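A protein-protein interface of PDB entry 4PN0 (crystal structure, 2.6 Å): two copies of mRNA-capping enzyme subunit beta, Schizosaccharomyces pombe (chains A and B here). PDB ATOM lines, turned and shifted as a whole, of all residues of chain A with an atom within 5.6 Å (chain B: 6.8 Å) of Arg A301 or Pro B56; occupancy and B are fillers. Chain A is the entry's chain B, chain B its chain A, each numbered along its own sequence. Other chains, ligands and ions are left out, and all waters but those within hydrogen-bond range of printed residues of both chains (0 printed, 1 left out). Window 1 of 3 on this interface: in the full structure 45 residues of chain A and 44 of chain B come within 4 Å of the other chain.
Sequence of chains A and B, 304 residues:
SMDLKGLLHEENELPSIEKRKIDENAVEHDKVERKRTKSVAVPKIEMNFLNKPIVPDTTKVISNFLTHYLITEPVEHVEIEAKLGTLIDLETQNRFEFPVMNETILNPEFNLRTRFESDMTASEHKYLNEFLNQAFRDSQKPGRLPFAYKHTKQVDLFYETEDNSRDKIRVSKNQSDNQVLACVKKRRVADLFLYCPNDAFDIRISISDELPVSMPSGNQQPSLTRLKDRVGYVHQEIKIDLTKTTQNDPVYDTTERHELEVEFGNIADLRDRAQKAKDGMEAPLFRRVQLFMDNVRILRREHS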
ATOM      1  N   ASP A 199     -27.350  24.356  15.608  1.00  0.00           N
ATOM      2  CA  ASP A 199     -26.536  25.509  15.255  1.00  0.00           C
ATOM      3  C   ASP A 199     -26.247  26.393  16.461  1.00  0.00           C
ATOM      4  O   ASP A 199     -26.761  26.162  17.554  1.00  0.00           O
ATOM      5  CB  ASP A 199     -27.224  26.317  14.156  1.00  0.00           C
ATOM      6  CG  ASP A 199     -27.704  25.445  13.017  1.00  0.00           C
ATOM      7  OD1 ASP A 199     -26.852  24.996  12.224  1.00  0.00           O
ATOM      8  OD2 ASP A 199     -28.928  25.203  12.919  1.00  0.00           O
ATOM      9  N   VAL A 296     -31.187  31.700   4.864  1.00  0.00           N
ATOM     10  CA  VAL A 296     -31.116  31.838   6.312  1.00  0.00           C
ATOM     11  C   VAL A 296     -30.373  30.658   6.935  1.00  0.00           C
ATOM     12  O   VAL A 296     -29.505  30.838   7.791  1.00  0.00           O
ATOM     13  CB  VAL A 296     -32.523  31.932   6.935  1.00  0.00           C
ATOM     14  CG1 VAL A 296     -32.426  32.032   8.434  1.00  0.00           C
ATOM     15  CG2 VAL A 296     -33.273  33.128   6.379  1.00  0.00           C
ATOM     16  N   ARG A 297     -30.715  29.453   6.491  1.00  0.00           N
ATOM     17  CA  ARG A 297     -30.092  28.239   7.006  1.00  0.00           C
ATOM     18  C   ARG A 297     -28.589  28.217   6.761  1.00  0.00           C
ATOM     19  O   ARG A 297     -27.824  27.788   7.624  1.00  0.00           O
ATOM     20  CB  ARG A 297     -30.746  26.995   6.401  1.00  0.00           C
ATOM     21  CG  ARG A 297     -32.175  26.784   6.858  1.00  0.00           C
ATOM     22  CD  ARG A 297     -32.747  25.465   6.367  1.00  0.00           C
ATOM     23  NE  ARG A 297     -34.085  25.247   6.910  1.00  0.00           N
ATOM     24  CZ  ARG A 297     -35.203  25.663   6.326  1.00  0.00           C
ATOM     25  NH1 ARG A 297     -35.146  26.310   5.170  1.00  0.00           N
ATOM     26  NH2 ARG A 297     -36.378  25.428   6.893  1.00  0.00           N
ATOM     27  N   ILE A 298     -28.169  28.680   5.587  1.00  0.00           N
ATOM     28  CA  ILE A 298     -26.751  28.721   5.253  1.00  0.00           C
ATOM     29  C   ILE A 298     -25.984  29.593   6.238  1.00  0.00           C
ATOM     30  O   ILE A 298     -24.964  29.173   6.786  1.00  0.00           O
ATOM     31  CB  ILE A 298     -26.518  29.258   3.833  1.00  0.00           C
ATOM     32  CG1 ILE A 298     -27.051  28.268   2.797  1.00  0.00           C
ATOM     33  CG2 ILE A 298     -25.040  29.518   3.603  1.00  0.00           C
ATOM     34  CD1 ILE A 298     -26.900  28.731   1.365  1.00  0.00           C
ATOM     35  N   LEU A 299     -26.492  30.801   6.465  1.00  0.00           N
ATOM     36  CA  LEU A 299     -25.852  31.767   7.354  1.00  0.00           C
ATOM     37  C   LEU A 299     -25.820  31.273   8.791  1.00  0.00           C
ATOM     38  O   LEU A 299     -24.799  31.374   9.472  1.00  0.00           O
ATOM     39  CB  LEU A 299     -26.580  33.107   7.284  1.00  0.00           C
ATOM     40  CG  LEU A 299     -26.553  33.764   5.906  1.00  0.00           C
ATOM     41  CD1 LEU A 299     -27.438  34.996   5.885  1.00  0.00           C
ATOM     42  CD2 LEU A 299     -25.123  34.112   5.532  1.00  0.00           C
ATOM     43  N   ARG A 300     -26.948  30.742   9.242  1.00  0.00           N
ATOM     44  CA  ARG A 300     -27.082  30.217  10.593  1.00  0.00           C
ATOM     45  C   ARG A 300     -26.057  29.130  10.886  1.00  0.00           C
ATOM     46  O   ARG A 300     -25.525  29.052  11.989  1.00  0.00           O
ATOM     47  CB  ARG A 300     -28.488  29.654  10.786  1.00  0.00           C
ATOM     48  CG  ARG A 300     -28.709  28.993  12.129  1.00  0.00           C
ATOM     49  CD  ARG A 300     -30.071  28.340  12.191  1.00  0.00           C
ATOM     50  NE  ARG A 300     -30.187  27.224  11.257  1.00  0.00           N
ATOM     51  CZ  ARG A 300     -31.333  26.821  10.719  1.00  0.00           C
ATOM     52  NH1 ARG A 300     -31.353  25.792   9.882  1.00  0.00           N
ATOM     53  NH2 ARG A 300     -32.461  27.451  11.015  1.00  0.00           N
ATOM     54  N   ARG A 301     -25.784  28.294   9.890  1.00  0.00           N
ATOM     55  CA  ARG A 301     -24.867  27.170  10.052  1.00  0.00           C
ATOM     56  C   ARG A 301     -23.411  27.610   9.993  1.00  0.00           C
ATOM     57  O   ARG A 301     -22.504  26.840  10.310  1.00  0.00           O
ATOM     58  CB  ARG A 301     -25.123  26.121   8.971  1.00  0.00           C
ATOM     59  CG  ARG A 301     -26.433  25.384   9.126  1.00  0.00           C
ATOM     60  CD  ARG A 301     -26.765  24.595   7.878  1.00  0.00           C
ATOM     61  NE  ARG A 301     -27.931  23.742   8.075  1.00  0.00           N
ATOM     62  CZ  ARG A 301     -28.446  22.957   7.136  1.00  0.00           C
ATOM     63  NH1 ARG A 301     -27.896  22.920   5.929  1.00  0.00           N
ATOM     64  NH2 ARG A 301     -29.508  22.210   7.402  1.00  0.00           N
ATOM     65  N   GLU A 302     -23.194  28.851   9.577  1.00  0.00           N
ATOM     66  CA  GLU A 302     -21.847  29.360   9.384  1.00  0.00           C
ATOM     67  C   GLU A 302     -21.255  29.899  10.685  1.00  0.00           C
ATOM     68  O   GLU A 302     -21.324  31.096  10.963  1.00  0.00           O
ATOM     69  CB  GLU A 302     -21.840  30.442   8.306  1.00  0.00           C
ATOM     70  CG  GLU A 302     -20.473  30.704   7.708  1.00  0.00           C
ATOM     71  CD  GLU A 302     -19.923  29.499   6.972  1.00  0.00           C
ATOM     72  OE1 GLU A 302     -20.729  28.691   6.460  1.00  0.00           O
ATOM     73  OE2 GLU A 302     -18.683  29.362   6.906  1.00  0.00           O
ATOM     74  N   HIS A 303     -20.676  29.001  11.477  1.00  0.00           N
ATOM     75  CA  HIS A 303     -20.032  29.367  12.732  1.00  0.00           C
ATOM     76  C   HIS A 303     -18.694  28.644  12.827  1.00  0.00           C
ATOM     77  O   HIS A 303     -18.535  27.551  12.282  1.00  0.00           O
ATOM     78  CB  HIS A 303     -20.923  28.987  13.916  1.00  0.00           C
ATOM     79  CG  HIS A 303     -20.463  29.541  15.228  1.00  0.00           C
ATOM     80  ND1 HIS A 303     -19.410  29.004  15.937  1.00  0.00           N
ATOM     81  CD2 HIS A 303     -20.922  30.580  15.969  1.00  0.00           C
ATOM     82  CE1 HIS A 303     -19.236  29.691  17.053  1.00  0.00           C
ATOM     83  NE2 HIS A 303     -20.141  30.652  17.096  1.00  0.00           N
ATOM     84  N   PRO B  53     -26.607  22.830  -3.360  1.00  0.00           N
ATOM     85  CA  PRO B  53     -27.722  22.116  -2.729  1.00  0.00           C
ATOM     86  C   PRO B  53     -27.685  22.261  -1.213  1.00  0.00           C
ATOM     87  O   PRO B  53     -26.656  21.991  -0.594  1.00  0.00           O
ATOM     88  CB  PRO B  53     -27.461  20.655  -3.112  1.00  0.00           C
ATOM     89  CG  PRO B  53     -26.656  20.732  -4.363  1.00  0.00           C
ATOM     90  CD  PRO B  53     -25.789  21.943  -4.204  1.00  0.00           C
ATOM     91  N   ILE B  54     -28.793  22.698  -0.624  1.00  0.00           N
ATOM     92  CA  ILE B  54     -28.874  22.846   0.822  1.00  0.00           C
ATOM     93  C   ILE B  54     -29.778  21.784   1.424  1.00  0.00           C
ATOM     94  O   ILE B  54     -30.915  21.599   0.990  1.00  0.00           O
ATOM     95  CB  ILE B  54     -29.365  24.247   1.232  1.00  0.00           C
ATOM     96  CG1 ILE B  54     -28.248  25.267   1.024  1.00  0.00           C
ATOM     97  CG2 ILE B  54     -29.801  24.262   2.690  1.00  0.00           C
ATOM     98  CD1 ILE B  54     -26.940  24.866   1.674  1.00  0.00           C
ATOM     99  N   VAL B  55     -29.255  21.086   2.425  1.00  0.00           N
ATOM    100  CA  VAL B  55     -29.975  20.002   3.069  1.00  0.00           C
ATOM    101  C   VAL B  55     -30.487  20.437   4.437  1.00  0.00           C
ATOM    102  O   VAL B  55     -29.715  20.911   5.267  1.00  0.00           O
ATOM    103  CB  VAL B  55     -29.067  18.769   3.219  1.00  0.00           C
ATOM    104  CG1 VAL B  55     -29.753  17.697   4.029  1.00  0.00           C
ATOM    105  CG2 VAL B  55     -28.672  18.238   1.850  1.00  0.00           C
ATOM    106  N   PRO B  56     -31.800  20.281   4.673  1.00  0.00           N
ATOM    107  CA  PRO B  56     -32.420  20.660   5.949  1.00  0.00           C
ATOM    108  C   PRO B  56     -31.903  19.810   7.104  1.00  0.00           C
ATOM    109  O   PRO B  56     -31.298  18.764   6.871  1.00  0.00           O
ATOM    110  CB  PRO B  56     -33.908  20.381   5.711  1.00  0.00           C
ATOM    111  CG  PRO B  56     -33.936  19.371   4.612  1.00  0.00           C
ATOM    112  CD  PRO B  56     -32.781  19.719   3.728  1.00  0.00           C
ATOM    113  N   ASP B  57     -32.143  20.261   8.332  1.00  0.00           N
ATOM    114  CA  ASP B  57     -31.657  19.565   9.521  1.00  0.00           C
ATOM    115  C   ASP B  57     -32.163  18.131   9.611  1.00  0.00           C
ATOM    116  O   ASP B  57     -31.396  17.217   9.913  1.00  0.00           O
ATOM    117  CB  ASP B  57     -32.043  20.331  10.791  1.00  0.00           C
ATOM    118  CG  ASP B  57     -31.062  21.434  11.129  1.00  0.00           C
ATOM    119  OD1 ASP B  57     -30.281  21.835  10.240  1.00  0.00           O
ATOM    120  OD2 ASP B  57     -31.075  21.903  12.288  1.00  0.00           O
ATOM    121  N   THR B  58     -33.452  17.943   9.346  1.00  0.00           N
ATOM    122  CA  THR B  58     -34.089  16.634   9.482  1.00  0.00           C
ATOM    123  C   THR B  58     -33.377  15.553   8.673  1.00  0.00           C
ATOM    124  O   THR B  58     -33.096  14.467   9.183  1.00  0.00           O
ATOM    125  CB  THR B  58     -35.569  16.681   9.061  1.00  0.00           C
ATOM    126  OG1 THR B  58     -36.282  17.581   9.917  1.00  0.00           O
ATOM    127  CG2 THR B  58     -36.190  15.301   9.168  1.00  0.00           C
ATOM    128  N   THR B  59     -33.082  15.861   7.416  1.00  0.00           N
ATOM    129  CA  THR B  59     -32.377  14.931   6.544  1.00  0.00           C
ATOM    130  C   THR B  59     -30.980  14.633   7.084  1.00  0.00           C
ATOM    131  O   THR B  59     -30.510  13.498   7.025  1.00  0.00           O
ATOM    132  CB  THR B  59     -32.274  15.484   5.109  1.00  0.00           C
ATOM    133  OG1 THR B  59     -33.588  15.674   4.570  1.00  0.00           O
ATOM    134  CG2 THR B  59     -31.502  14.530   4.212  1.00  0.00           C
ATOM    135  N   LYS B  60     -30.322  15.654   7.623  1.00  0.00           N
ATOM    136  CA  LYS B  60     -28.980  15.483   8.168  1.00  0.00           C
ATOM    137  C   LYS B  60     -28.972  14.613   9.420  1.00  0.00           C
ATOM    138  O   LYS B  60     -28.113  13.747   9.575  1.00  0.00           O
ATOM    139  CB  LYS B  60     -28.324  16.836   8.454  1.00  0.00           C
ATOM    140  CG  LYS B  60     -27.908  17.587   7.203  1.00  0.00           C
ATOM    141  CD  LYS B  60     -26.887  18.673   7.503  1.00  0.00           C
ATOM    142  CE  LYS B  60     -26.438  19.356   6.219  1.00  0.00           C
ATOM    143  NZ  LYS B  60     -25.342  20.339   6.443  1.00  0.00           N
ATOM    144  N   VAL B  61     -29.928  14.846  10.313  1.00  0.00           N
ATOM    145  CA  VAL B  61     -30.015  14.064  11.539  1.00  0.00           C
ATOM    146  C   VAL B  61     -30.296  12.599  11.223  1.00  0.00           C
ATOM    147  O   VAL B  61     -29.613  11.704  11.724  1.00  0.00           O
ATOM    148  CB  VAL B  61     -31.103  14.602  12.482  1.00  0.00           C
ATOM    149  CG1 VAL B  61     -31.193  13.738  13.731  1.00  0.00           C
ATOM    150  CG2 VAL B  61     -30.814  16.046  12.852  1.00  0.00           C
ATOM    151  N   GLN B 290     -33.449  11.943   1.579  1.00  0.00           N
ATOM    152  CA  GLN B 290     -34.428  12.946   1.186  1.00  0.00           C
ATOM    153  C   GLN B 290     -35.583  12.287   0.444  1.00  0.00           C
ATOM    154  O   GLN B 290     -36.745  12.510   0.772  1.00  0.00           O
ATOM    155  CB  GLN B 290     -33.783  14.010   0.299  1.00  0.00           C
ATOM    156  CG  GLN B 290     -34.728  15.126  -0.114  1.00  0.00           C
ATOM    157  CD  GLN B 290     -35.111  16.018   1.049  1.00  0.00           C
ATOM    158  OE1 GLN B 290     -34.261  16.412   1.849  1.00  0.00           O
ATOM    159  NE2 GLN B 290     -36.397  16.340   1.151  1.00  0.00           N
ATOM    160  N   ARG B 297     -43.359  11.524   3.778  1.00  0.00           N
ATOM    161  CA  ARG B 297     -44.140  12.743   3.958  1.00  0.00           C
ATOM    162  C   ARG B 297     -45.476  12.657   3.223  1.00  0.00           C
ATOM    163  O   ARG B 297     -46.532  12.907   3.804  1.00  0.00           O
ATOM    164  CB  ARG B 297     -43.352  13.956   3.460  1.00  0.00           C
ATOM    165  CG  ARG B 297     -43.209  15.062   4.487  1.00  0.00           C
ATOM    166  CD  ARG B 297     -42.352  16.208   3.964  1.00  0.00           C
ATOM    167  NE  ARG B 297     -40.994  15.780   3.635  1.00  0.00           N
ATOM    168  CZ  ARG B 297     -40.011  15.662   4.523  1.00  0.00           C
ATOM    169  NH1 ARG B 297     -40.234  15.933   5.803  1.00  0.00           N
ATOM    170  NH2 ARG B 297     -38.806  15.269   4.134  1.00  0.00           N
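OD2 of Asp A199 lies within salt-bridge range of NE of Arg A300 (2.9 Å).
Among the printed residues, merely in contact across the chains: Arg A301 with Pro B56 (3.4 Å), Ile A298 with Ile B54 (3.6 Å), Arg A301 with Lys B60 (3.7 Å), Asp A199 with Asp B57 (3.99 Å) and Arg A301 with Ile B54 (3.99 Å).
Of the printed residues of chain B, Arg A301 touches Ile B54, Val B55, Pro B56, Asp B57 and Lys B60. Of chain A, only Arg A301 (3.4 Å) comes within 4 Å of Pro B56. Of the printed residues of chain A, Val B55 touches Arg A301 (2.5 Å). Printed residues of chain A within 4 Å of Asp B57: Asp A199 (3.99 Å) and Arg A301 (3.0 Å). Leu A299 touches none of the printed residues of chain B. The nearest printed residue of chain B that does not touch Arg A301 is Thr B58 (6.1 Å).
Position printed for both chains: 297.
OD1 of Asp B57 lies within salt-bridge range of NH2 of Arg A301, at 3.0 Å. The backbone carbonyl oxygen of Val B55 sits at hydrogen-bond distance from the guanidinium group of Arg A301, at 2.5 Å.
Of the 11 printed residues of chain B, 5 touch a printed residue of chain A. Printed residues of chain B that touch a printed residue of chain A: Ile B54, Val B55, Pro B56, Asp B57 and Lys B60. Hydrophobic or aromatic side chains of chain B within 4 Å of the printed part of chain A: Ile B54. Printed residues of chain A that touch a printed residue of chain B: Asp A199, Ile A298 and Arg A301. Hydrophobic or aromatic side chains of chain A that line the printed part of chain B: Ile A298. Among the printed residues, Asp or Glu carboxylates within 4 Å of a Lys or Arg side-chain nitrogen of the other chain: Arg A301 with Asp B57.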
